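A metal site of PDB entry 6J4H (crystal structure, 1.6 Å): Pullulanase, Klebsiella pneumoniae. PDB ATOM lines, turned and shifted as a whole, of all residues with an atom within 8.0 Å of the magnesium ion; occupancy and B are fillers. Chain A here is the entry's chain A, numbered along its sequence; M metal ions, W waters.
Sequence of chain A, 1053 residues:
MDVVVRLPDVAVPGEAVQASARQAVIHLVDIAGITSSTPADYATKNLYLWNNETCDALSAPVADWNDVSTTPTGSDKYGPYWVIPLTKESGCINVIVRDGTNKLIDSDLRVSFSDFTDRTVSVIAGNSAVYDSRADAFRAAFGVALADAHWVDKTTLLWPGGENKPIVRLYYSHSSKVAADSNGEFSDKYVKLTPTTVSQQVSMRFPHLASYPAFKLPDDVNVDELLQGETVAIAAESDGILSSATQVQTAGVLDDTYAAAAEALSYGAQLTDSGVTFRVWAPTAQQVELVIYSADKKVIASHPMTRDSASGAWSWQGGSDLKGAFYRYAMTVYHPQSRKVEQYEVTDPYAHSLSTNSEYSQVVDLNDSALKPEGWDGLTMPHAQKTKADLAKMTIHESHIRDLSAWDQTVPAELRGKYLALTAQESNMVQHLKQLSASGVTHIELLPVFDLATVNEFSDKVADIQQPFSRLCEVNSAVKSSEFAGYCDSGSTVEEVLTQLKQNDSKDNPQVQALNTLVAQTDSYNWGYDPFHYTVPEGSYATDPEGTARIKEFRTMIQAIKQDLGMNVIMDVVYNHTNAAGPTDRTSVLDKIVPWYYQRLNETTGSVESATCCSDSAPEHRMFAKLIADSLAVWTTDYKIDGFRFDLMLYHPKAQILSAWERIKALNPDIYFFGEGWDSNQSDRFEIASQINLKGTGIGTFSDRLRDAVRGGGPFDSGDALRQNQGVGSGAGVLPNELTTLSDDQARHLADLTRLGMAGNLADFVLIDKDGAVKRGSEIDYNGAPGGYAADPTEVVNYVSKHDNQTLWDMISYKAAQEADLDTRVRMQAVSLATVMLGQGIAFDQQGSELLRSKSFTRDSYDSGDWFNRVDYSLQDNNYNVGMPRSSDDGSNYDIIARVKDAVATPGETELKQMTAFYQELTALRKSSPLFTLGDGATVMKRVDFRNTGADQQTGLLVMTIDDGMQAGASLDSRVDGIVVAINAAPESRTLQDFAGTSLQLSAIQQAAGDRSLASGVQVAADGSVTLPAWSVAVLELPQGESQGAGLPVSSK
OG of Ser 358 sits at hydrogen-bond distance from OD2 of Asp 451 (2.6 Å).
O of Asp 451 sits at hydrogen-bond distance from N of Phe 532, 2.9 Å away.
The side-chain carboxylate (OD2) of Asp 451 sits at hydrogen-bond distance from a ring nitrogen (ND1) of His 533 (2.9 Å).
The backbone NH (N) of Asp 451 lies within hydrogen-bond range of the backbone carbonyl oxygen (O) of Val 536 (2.8 Å).
The side-chain carboxylate of Glu 457 lies close to the backbone NH of Gly 539 (2.9 Å).
The backbone NH of Glu 457 lies within hydrogen-bond range of the side-chain amide oxygen of Asn 357, at 2.9 Å.
The side-chain carboxylate (OE1) of Glu 457 lies within salt-bridge range of the guanidinium group (NH2) of Arg 550 (3.6 Å).
OG of Ser 540 sits at hydrogen-bond distance from OE1 of Glu 538.
Ser 358 touches the magnesium ion (OG to MG, 3.98 Å).
Of the 26 residues printed, 5 come within 4 Å of the magnesium ion.
The nearest printed residue that does not touch the magnesium ion is Gly 539 (4.3 Å).
The magnesium ion is bound by the side-chain carboxylate of Asp 451 (2.1 Å), the side-chain carboxylate of Glu 457 (2.2 Å), water W2 (2.2 Å), the backbone carbonyl oxygen of Leu 452 (2.2 Å), water W1 (2.3 Å) and the side-chain carboxylate of Glu 538 (2.3 Å).
The magnesium ion has six donor atoms within binding distance.
Water W2 bridges the backbone carbonyl oxygen (O) of Val 455 (2.6 Å) and the side-chain carboxylate (OE1) of Glu 538 (2.7 Å).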
ATOM      1  N   LEU A 354      10.985  23.820 -15.530  1.00  0.00           N
ATOM      2  CA  LEU A 354      10.074  24.928 -15.255  1.00  0.00           C
ATOM      3  C   LEU A 354      10.317  26.072 -16.225  1.00  0.00           C
ATOM      4  O   LEU A 354      11.431  26.237 -16.750  1.00  0.00           O
ATOM      5  CB  LEU A 354      10.244  25.461 -13.818  1.00  0.00           C
ATOM      6  CG  LEU A 354       9.864  24.521 -12.676  1.00  0.00           C
ATOM      7  CD1 LEU A 354      10.507  24.988 -11.376  1.00  0.00           C
ATOM      8  CD2 LEU A 354       8.346  24.410 -12.536  1.00  0.00           C
ATOM      9  N   SER A 355       9.283  26.875 -16.432  1.00  0.00           N
ATOM     10  CA  SER A 355       9.457  28.173 -17.065  1.00  0.00           C
ATOM     11  C   SER A 355      10.048  29.164 -16.066  1.00  0.00           C
ATOM     12  O   SER A 355      10.277  28.856 -14.891  1.00  0.00           O
ATOM     13  CB  SER A 355       8.120  28.689 -17.596  1.00  0.00           C
ATOM     14  OG  SER A 355       7.254  29.043 -16.523  1.00  0.00           O
ATOM     15  N   THR A 356      10.285  30.391 -16.534  1.00  0.00           N
ATOM     16  CA  THR A 356      10.823  31.431 -15.671  1.00  0.00           C
ATOM     17  C   THR A 356       9.916  31.679 -14.478  1.00  0.00           C
ATOM     18  O   THR A 356       8.704  31.873 -14.622  1.00  0.00           O
ATOM     19  CB  THR A 356      11.001  32.727 -16.474  1.00  0.00           C
ATOM     20  OG1 THR A 356      11.895  32.501 -17.568  1.00  0.00           O
ATOM     21  CG2 THR A 356      11.609  33.807 -15.574  1.00  0.00           C
ATOM     22  N   ASN A 357      10.521  31.717 -13.276  1.00  0.00           N
ATOM     23  CA  ASN A 357       9.833  31.961 -12.014  1.00  0.00           C
ATOM     24  C   ASN A 357       8.821  30.878 -11.678  1.00  0.00           C
ATOM     25  O   ASN A 357       7.912  31.106 -10.860  1.00  0.00           O
ATOM     26  CB  ASN A 357       9.161  33.355 -12.003  1.00  0.00           C
ATOM     27  CG  ASN A 357       9.209  34.008 -10.626  1.00  0.00           C
ATOM     28  OD1 ASN A 357      10.186  33.833  -9.873  1.00  0.00           O
ATOM     29  ND2 ASN A 357       8.148  34.735 -10.268  1.00  0.00           N
ATOM     30  N   SER A 358       8.965  29.709 -12.290  1.00  0.00           N
ATOM     31  CA  SER A 358       8.218  28.503 -11.919  1.00  0.00           C
ATOM     32  C   SER A 358       6.723  28.600 -12.225  1.00  0.00           C
ATOM     33  O   SER A 358       5.921  27.899 -11.590  1.00  0.00           O
ATOM     34  CB  SER A 358       8.407  28.172 -10.434  1.00  0.00           C
ATOM     35  OG  SER A 358       9.759  28.361 -10.021  1.00  0.00           O
ATOM     36  N   PHE A 450      17.761  23.709  -5.227  1.00  0.00           N
ATOM     37  CA  PHE A 450      16.454  23.380  -5.774  1.00  0.00           C
ATOM     38  C   PHE A 450      15.671  24.679  -5.978  1.00  0.00           C
ATOM     39  O   PHE A 450      16.136  25.760  -5.619  1.00  0.00           O
ATOM     40  CB  PHE A 450      15.706  22.438  -4.825  1.00  0.00           C
ATOM     41  CG  PHE A 450      15.587  22.987  -3.430  1.00  0.00           C
ATOM     42  CD1 PHE A 450      14.547  23.842  -3.100  1.00  0.00           C
ATOM     43  CD2 PHE A 450      16.552  22.682  -2.478  1.00  0.00           C
ATOM     44  CE1 PHE A 450      14.464  24.375  -1.825  1.00  0.00           C
ATOM     45  CE2 PHE A 450      16.474  23.204  -1.196  1.00  0.00           C
ATOM     46  CZ  PHE A 450      15.421  24.061  -0.866  1.00  0.00           C
ATOM     47  N   ASP A 451      14.475  24.586  -6.551  1.00  0.00           N
ATOM     48  CA  ASP A 451      13.748  25.805  -6.930  1.00  0.00           C
ATOM     49  C   ASP A 451      13.172  26.477  -5.696  1.00  0.00           C
ATOM     50  O   ASP A 451      12.151  26.044  -5.160  1.00  0.00           O
ATOM     51  CB  ASP A 451      12.653  25.472  -7.924  1.00  0.00           C
ATOM     52  CG  ASP A 451      11.789  26.693  -8.256  1.00  0.00           C
ATOM     53  OD1 ASP A 451      12.336  27.811  -8.341  1.00  0.00           O
ATOM     54  OD2 ASP A 451      10.571  26.523  -8.434  1.00  0.00           O
ATOM     55  N   LEU A 452      13.821  27.559  -5.248  1.00  0.00           N
ATOM     56  CA  LEU A 452      13.287  28.376  -4.169  1.00  0.00           C
ATOM     57  C   LEU A 452      12.290  29.405  -4.709  1.00  0.00           C
ATOM     58  O   LEU A 452      12.221  29.677  -5.915  1.00  0.00           O
ATOM     59  CB  LEU A 452      14.433  29.075  -3.417  1.00  0.00           C
ATOM     60  CG  LEU A 452      15.404  29.860  -4.296  1.00  0.00           C
ATOM     61  CD1 LEU A 452      15.321  31.363  -3.982  1.00  0.00           C
ATOM     62  CD2 LEU A 452      16.827  29.380  -4.103  1.00  0.00           C
ATOM     63  N   ALA A 453      11.505  29.968  -3.791  1.00  0.00           N
ATOM     64  CA  ALA A 453      10.425  30.859  -4.191  1.00  0.00           C
ATOM     65  C   ALA A 453      10.757  32.336  -4.007  1.00  0.00           C
ATOM     66  O   ALA A 453      10.090  33.170  -4.637  1.00  0.00           O
ATOM     67  CB  ALA A 453       9.153  30.558  -3.385  1.00  0.00           C
ATOM     68  N   THR A 454      11.756  32.664  -3.200  1.00  0.00           N
ATOM     69  CA  THR A 454      11.919  33.996  -2.631  1.00  0.00           C
ATOM     70  C   THR A 454      12.896  34.881  -3.404  1.00  0.00           C
ATOM     71  O   THR A 454      13.342  35.914  -2.897  1.00  0.00           O
ATOM     72  CB  THR A 454      12.348  33.869  -1.176  1.00  0.00           C
ATOM     73  OG1 THR A 454      13.324  32.822  -1.061  1.00  0.00           O
ATOM     74  CG2 THR A 454      11.138  33.518  -0.313  1.00  0.00           C
ATOM     75  N   VAL A 455      13.245  34.489  -4.631  1.00  0.00           N
ATOM     76  CA  VAL A 455      13.876  35.368  -5.604  1.00  0.00           C
ATOM     77  C   VAL A 455      12.993  35.385  -6.857  1.00  0.00           C
ATOM     78  O   VAL A 455      12.548  34.321  -7.314  1.00  0.00           O
ATOM     79  CB  VAL A 455      15.312  34.935  -5.955  1.00  0.00           C
ATOM     80  CG1 VAL A 455      15.897  35.822  -7.036  1.00  0.00           C
ATOM     81  CG2 VAL A 455      16.206  34.987  -4.703  1.00  0.00           C
ATOM     82  N   ASN A 456      12.710  36.574  -7.380  1.00  0.00           N
ATOM     83  CA  ASN A 456      11.946  36.663  -8.609  1.00  0.00           C
ATOM     84  C   ASN A 456      12.876  36.340  -9.765  1.00  0.00           C
ATOM     85  O   ASN A 456      13.927  36.971  -9.927  1.00  0.00           O
ATOM     86  CB  ASN A 456      11.334  38.057  -8.766  1.00  0.00           C
ATOM     87  CG  ASN A 456      10.282  38.112  -9.839  1.00  0.00           C
ATOM     88  OD1 ASN A 456      10.434  37.508 -10.900  1.00  0.00           O
ATOM     89  ND2 ASN A 456       9.203  38.842  -9.587  1.00  0.00           N
ATOM     90  N   GLU A 457      12.525  35.321 -10.553  1.00  0.00           N
ATOM     91  CA  GLU A 457      13.409  34.894 -11.625  1.00  0.00           C
ATOM     92  C   GLU A 457      13.245  35.728 -12.907  1.00  0.00           C
ATOM     93  O   GLU A 457      14.017  35.521 -13.856  1.00  0.00           O
ATOM     94  CB  GLU A 457      13.206  33.406 -11.904  1.00  0.00           C
ATOM     95  CG  GLU A 457      13.424  32.544 -10.663  1.00  0.00           C
ATOM     96  CD  GLU A 457      13.328  31.050 -10.946  1.00  0.00           C
ATOM     97  OE1 GLU A 457      12.896  30.681 -12.058  1.00  0.00           O
ATOM     98  OE2 GLU A 457      13.678  30.246 -10.042  1.00  0.00           O
ATOM     99  N   ASP A 530      13.052  28.019   1.132  1.00  0.00           N
ATOM    100  CA  ASP A 530      11.697  28.448   0.771  1.00  0.00           C
ATOM    101  C   ASP A 530      11.273  27.622  -0.430  1.00  0.00           C
ATOM    102  O   ASP A 530      11.272  28.106  -1.572  1.00  0.00           O
ATOM    103  CB  ASP A 530      11.673  29.950   0.450  1.00  0.00           C
ATOM    104  CG  ASP A 530      12.225  30.806   1.576  1.00  0.00           C
ATOM    105  OD1 ASP A 530      11.640  30.770   2.672  1.00  0.00           O
ATOM    106  OD2 ASP A 530      13.210  31.549   1.341  1.00  0.00           O
ATOM    107  N   PRO A 531      10.929  26.351  -0.226  1.00  0.00           N
ATOM    108  CA  PRO A 531      10.810  25.426  -1.369  1.00  0.00           C
ATOM    109  C   PRO A 531       9.579  25.702  -2.214  1.00  0.00           C
ATOM    110  O   PRO A 531       8.462  25.740  -1.697  1.00  0.00           O
ATOM    111  CB  PRO A 531      10.724  24.054  -0.705  1.00  0.00           C
ATOM    112  CG  PRO A 531      11.295  24.259   0.680  1.00  0.00           C
ATOM    113  CD  PRO A 531      10.876  25.643   1.057  1.00  0.00           C
ATOM    114  N   PHE A 532       9.794  25.857  -3.511  1.00  0.00           N
ATOM    115  CA  PHE A 532       8.740  26.004  -4.500  1.00  0.00           C
ATOM    116  C   PHE A 532       8.545  24.707  -5.268  1.00  0.00           C
ATOM    117  O   PHE A 532       7.417  24.178  -5.349  1.00  0.00           O
ATOM    118  CB  PHE A 532       9.088  27.182  -5.439  1.00  0.00           C
ATOM    119  CG  PHE A 532       7.904  27.815  -6.151  1.00  0.00           C
ATOM    120  CD1 PHE A 532       6.660  27.204  -6.164  1.00  0.00           C
ATOM    121  CD2 PHE A 532       8.072  29.033  -6.805  1.00  0.00           C
ATOM    122  CE1 PHE A 532       5.592  27.809  -6.823  1.00  0.00           C
ATOM    123  CE2 PHE A 532       7.011  29.637  -7.457  1.00  0.00           C
ATOM    124  CZ  PHE A 532       5.774  29.024  -7.477  1.00  0.00           C
ATOM    125  N   HIS A 533       9.629  24.147  -5.804  1.00  0.00           N
ATOM    126  CA  HIS A 533       9.617  22.811  -6.405  1.00  0.00           C
ATOM    127  C   HIS A 533      10.860  22.056  -5.946  1.00  0.00           C
ATOM    128  O   HIS A 533      11.976  22.566  -6.063  1.00  0.00           O
ATOM    129  CB  HIS A 533       9.565  22.867  -7.934  1.00  0.00           C
ATOM    130  CG  HIS A 533       8.321  23.521  -8.435  1.00  0.00           C
ATOM    131  ND1 HIS A 533       8.185  24.889  -8.546  1.00  0.00           N
ATOM    132  CD2 HIS A 533       7.136  22.991  -8.836  1.00  0.00           C
ATOM    133  CE1 HIS A 533       6.974  25.173  -9.009  1.00  0.00           C
ATOM    134  NE2 HIS A 533       6.316  24.033  -9.181  1.00  0.00           N
ATOM    135  N   VAL A 536      13.579  20.531  -9.208  1.00  0.00           N
ATOM    136  CA  VAL A 536      14.065  21.332 -10.333  1.00  0.00           C
ATOM    137  C   VAL A 536      15.157  22.243  -9.788  1.00  0.00           C
ATOM    138  O   VAL A 536      15.003  22.756  -8.670  1.00  0.00           O
ATOM    139  CB  VAL A 536      12.948  22.178 -10.952  1.00  0.00           C
ATOM    140  CG1 VAL A 536      13.425  22.849 -12.225  1.00  0.00           C
ATOM    141  CG2 VAL A 536      11.713  21.352 -11.240  1.00  0.00           C
ATOM    142  N   PRO A 537      16.240  22.493 -10.520  1.00  0.00           N
ATOM    143  CA  PRO A 537      17.201  23.515 -10.071  1.00  0.00           C
ATOM    144  C   PRO A 537      16.567  24.893  -9.989  1.00  0.00           C
ATOM    145  O   PRO A 537      15.602  25.198 -10.679  1.00  0.00           O
ATOM    146  CB  PRO A 537      18.301  23.458 -11.140  1.00  0.00           C
ATOM    147  CG  PRO A 537      18.207  22.065 -11.714  1.00  0.00           C
ATOM    148  CD  PRO A 537      16.718  21.756 -11.699  1.00  0.00           C
ATOM    149  N   GLU A 538      17.122  25.727  -9.117  1.00  0.00           N
ATOM    150  CA  GLU A 538      16.705  27.121  -9.030  1.00  0.00           C
ATOM    151  C   GLU A 538      17.000  27.861 -10.342  1.00  0.00           C
ATOM    152  O   GLU A 538      18.060  27.670 -10.952  1.00  0.00           O
ATOM    153  CB  GLU A 538      17.421  27.798  -7.849  1.00  0.00           C
ATOM    154  CG  GLU A 538      17.432  29.336  -7.879  1.00  0.00           C
ATOM    155  CD  GLU A 538      16.049  29.973  -7.825  1.00  0.00           C
ATOM    156  OE1 GLU A 538      15.971  31.200  -8.025  1.00  0.00           O
ATOM    157  OE2 GLU A 538      15.029  29.275  -7.591  1.00  0.00           O
ATOM    158  N   GLY A 539      16.055  28.690 -10.781  1.00  0.00           N
ATOM    159  CA  GLY A 539      16.210  29.412 -12.033  1.00  0.00           C
ATOM    160  C   GLY A 539      17.092  30.638 -11.991  1.00  0.00           C
ATOM    161  O   GLY A 539      17.813  30.915 -12.958  1.00  0.00           O
ATOM    162  N   SER A 540      17.072  31.403 -10.892  1.00  0.00           N
ATOM    163  CA  SER A 540      17.830  32.649 -10.881  1.00  0.00           C
ATOM    164  C   SER A 540      19.342  32.427 -10.899  1.00  0.00           C
ATOM    165  O   SER A 540      20.079  33.352 -11.247  1.00  0.00           O
ATOM    166  CB  SER A 540      17.442  33.503  -9.672  1.00  0.00           C
ATOM    167  OG  SER A 540      17.967  32.946  -8.482  1.00  0.00           O
ATOM    168  N   TYR A 541      19.815  31.228 -10.541  1.00  0.00           N
ATOM    169  CA  TYR A 541      21.236  30.920 -10.610  1.00  0.00           C
ATOM    170  C   TYR A 541      21.671  30.462 -11.998  1.00  0.00           C
ATOM    171  O   TYR A 541      22.861  30.211 -12.215  1.00  0.00           O
ATOM    172  CB  TYR A 541      21.604  29.850  -9.584  1.00  0.00           C
ATOM    173  CG  TYR A 541      21.328  30.231  -8.136  1.00  0.00           C
ATOM    174  CD1 TYR A 541      21.499  31.552  -7.701  1.00  0.00           C
ATOM    175  CD2 TYR A 541      20.922  29.275  -7.206  1.00  0.00           C
ATOM    176  CE1 TYR A 541      21.264  31.906  -6.379  1.00  0.00           C
ATOM    177  CE2 TYR A 541      20.692  29.619  -5.877  1.00  0.00           C
ATOM    178  CZ  TYR A 541      20.863  30.929  -5.470  1.00  0.00           C
ATOM    179  OH  TYR A 541      20.619  31.274  -4.156  1.00  0.00           O
ATOM    180  N   PRO A 545      16.741  31.463 -17.196  1.00  0.00           N
ATOM    181  CA  PRO A 545      15.798  30.714 -16.366  1.00  0.00           C
ATOM    182  C   PRO A 545      14.610  30.154 -17.127  1.00  0.00           C
ATOM    183  O   PRO A 545      13.713  29.569 -16.509  1.00  0.00           O
ATOM    184  CB  PRO A 545      15.345  31.761 -15.357  1.00  0.00           C
ATOM    185  CG  PRO A 545      15.318  33.030 -16.179  1.00  0.00           C
ATOM    186  CD  PRO A 545      16.506  32.919 -17.104  1.00  0.00           C
ATOM    187  N   ARG A 550      18.667  25.676 -17.489  1.00  0.00           N
ATOM    188  CA  ARG A 550      19.281  25.611 -16.158  1.00  0.00           C
ATOM    189  C   ARG A 550      19.789  24.224 -15.819  1.00  0.00           C
ATOM    190  O   ARG A 550      20.712  24.078 -15.011  1.00  0.00           O
ATOM    191  CB  ARG A 550      18.281  26.066 -15.096  1.00  0.00           C
ATOM    192  CG  ARG A 550      17.110  25.089 -14.900  1.00  0.00           C
ATOM    193  CD  ARG A 550      16.155  25.599 -13.858  1.00  0.00           C
ATOM    194  NE  ARG A 550      15.243  26.615 -14.410  1.00  0.00           N
ATOM    195  CZ  ARG A 550      14.182  27.069 -13.759  1.00  0.00           C
ATOM    196  NH1 ARG A 550      13.912  26.608 -12.540  1.00  0.00           N
ATOM    197  NH2 ARG A 550      13.371  27.957 -14.329  1.00  0.00           N
ATOM    198  N   ARG A 586       0.432  32.011  -4.541  1.00  0.00           N
ATOM    199  CA  ARG A 586       1.126  31.675  -5.781  1.00  0.00           C
ATOM    200  C   ARG A 586       2.032  30.467  -5.625  1.00  0.00           C
ATOM    201  O   ARG A 586       2.178  29.662  -6.557  1.00  0.00           O
ATOM    202  CB  ARG A 586       1.950  32.899  -6.235  1.00  0.00           C
ATOM    203  CG  ARG A 586       3.076  32.616  -7.225  1.00  0.00           C
ATOM    204  CD  ARG A 586       3.967  33.850  -7.465  1.00  0.00           C
ATOM    205  NE  ARG A 586       4.883  34.111  -6.355  1.00  0.00           N
ATOM    206  CZ  ARG A 586       6.182  33.772  -6.342  1.00  0.00           C
ATOM    207  NH1 ARG A 586       6.733  33.155  -7.379  1.00  0.00           N
ATOM    208  NH2 ARG A 586       6.930  34.049  -5.278  1.00  0.00           N
HETATM  209 MG    MG M   1      12.893  29.819  -8.057  1.00  0.00          MG
HETATM  210  O   HOH W   1      10.866  30.567  -8.691  1.00  0.00           O
HETATM  211  O   HOH W   2      13.438  31.860  -7.355  1.00  0.00           O
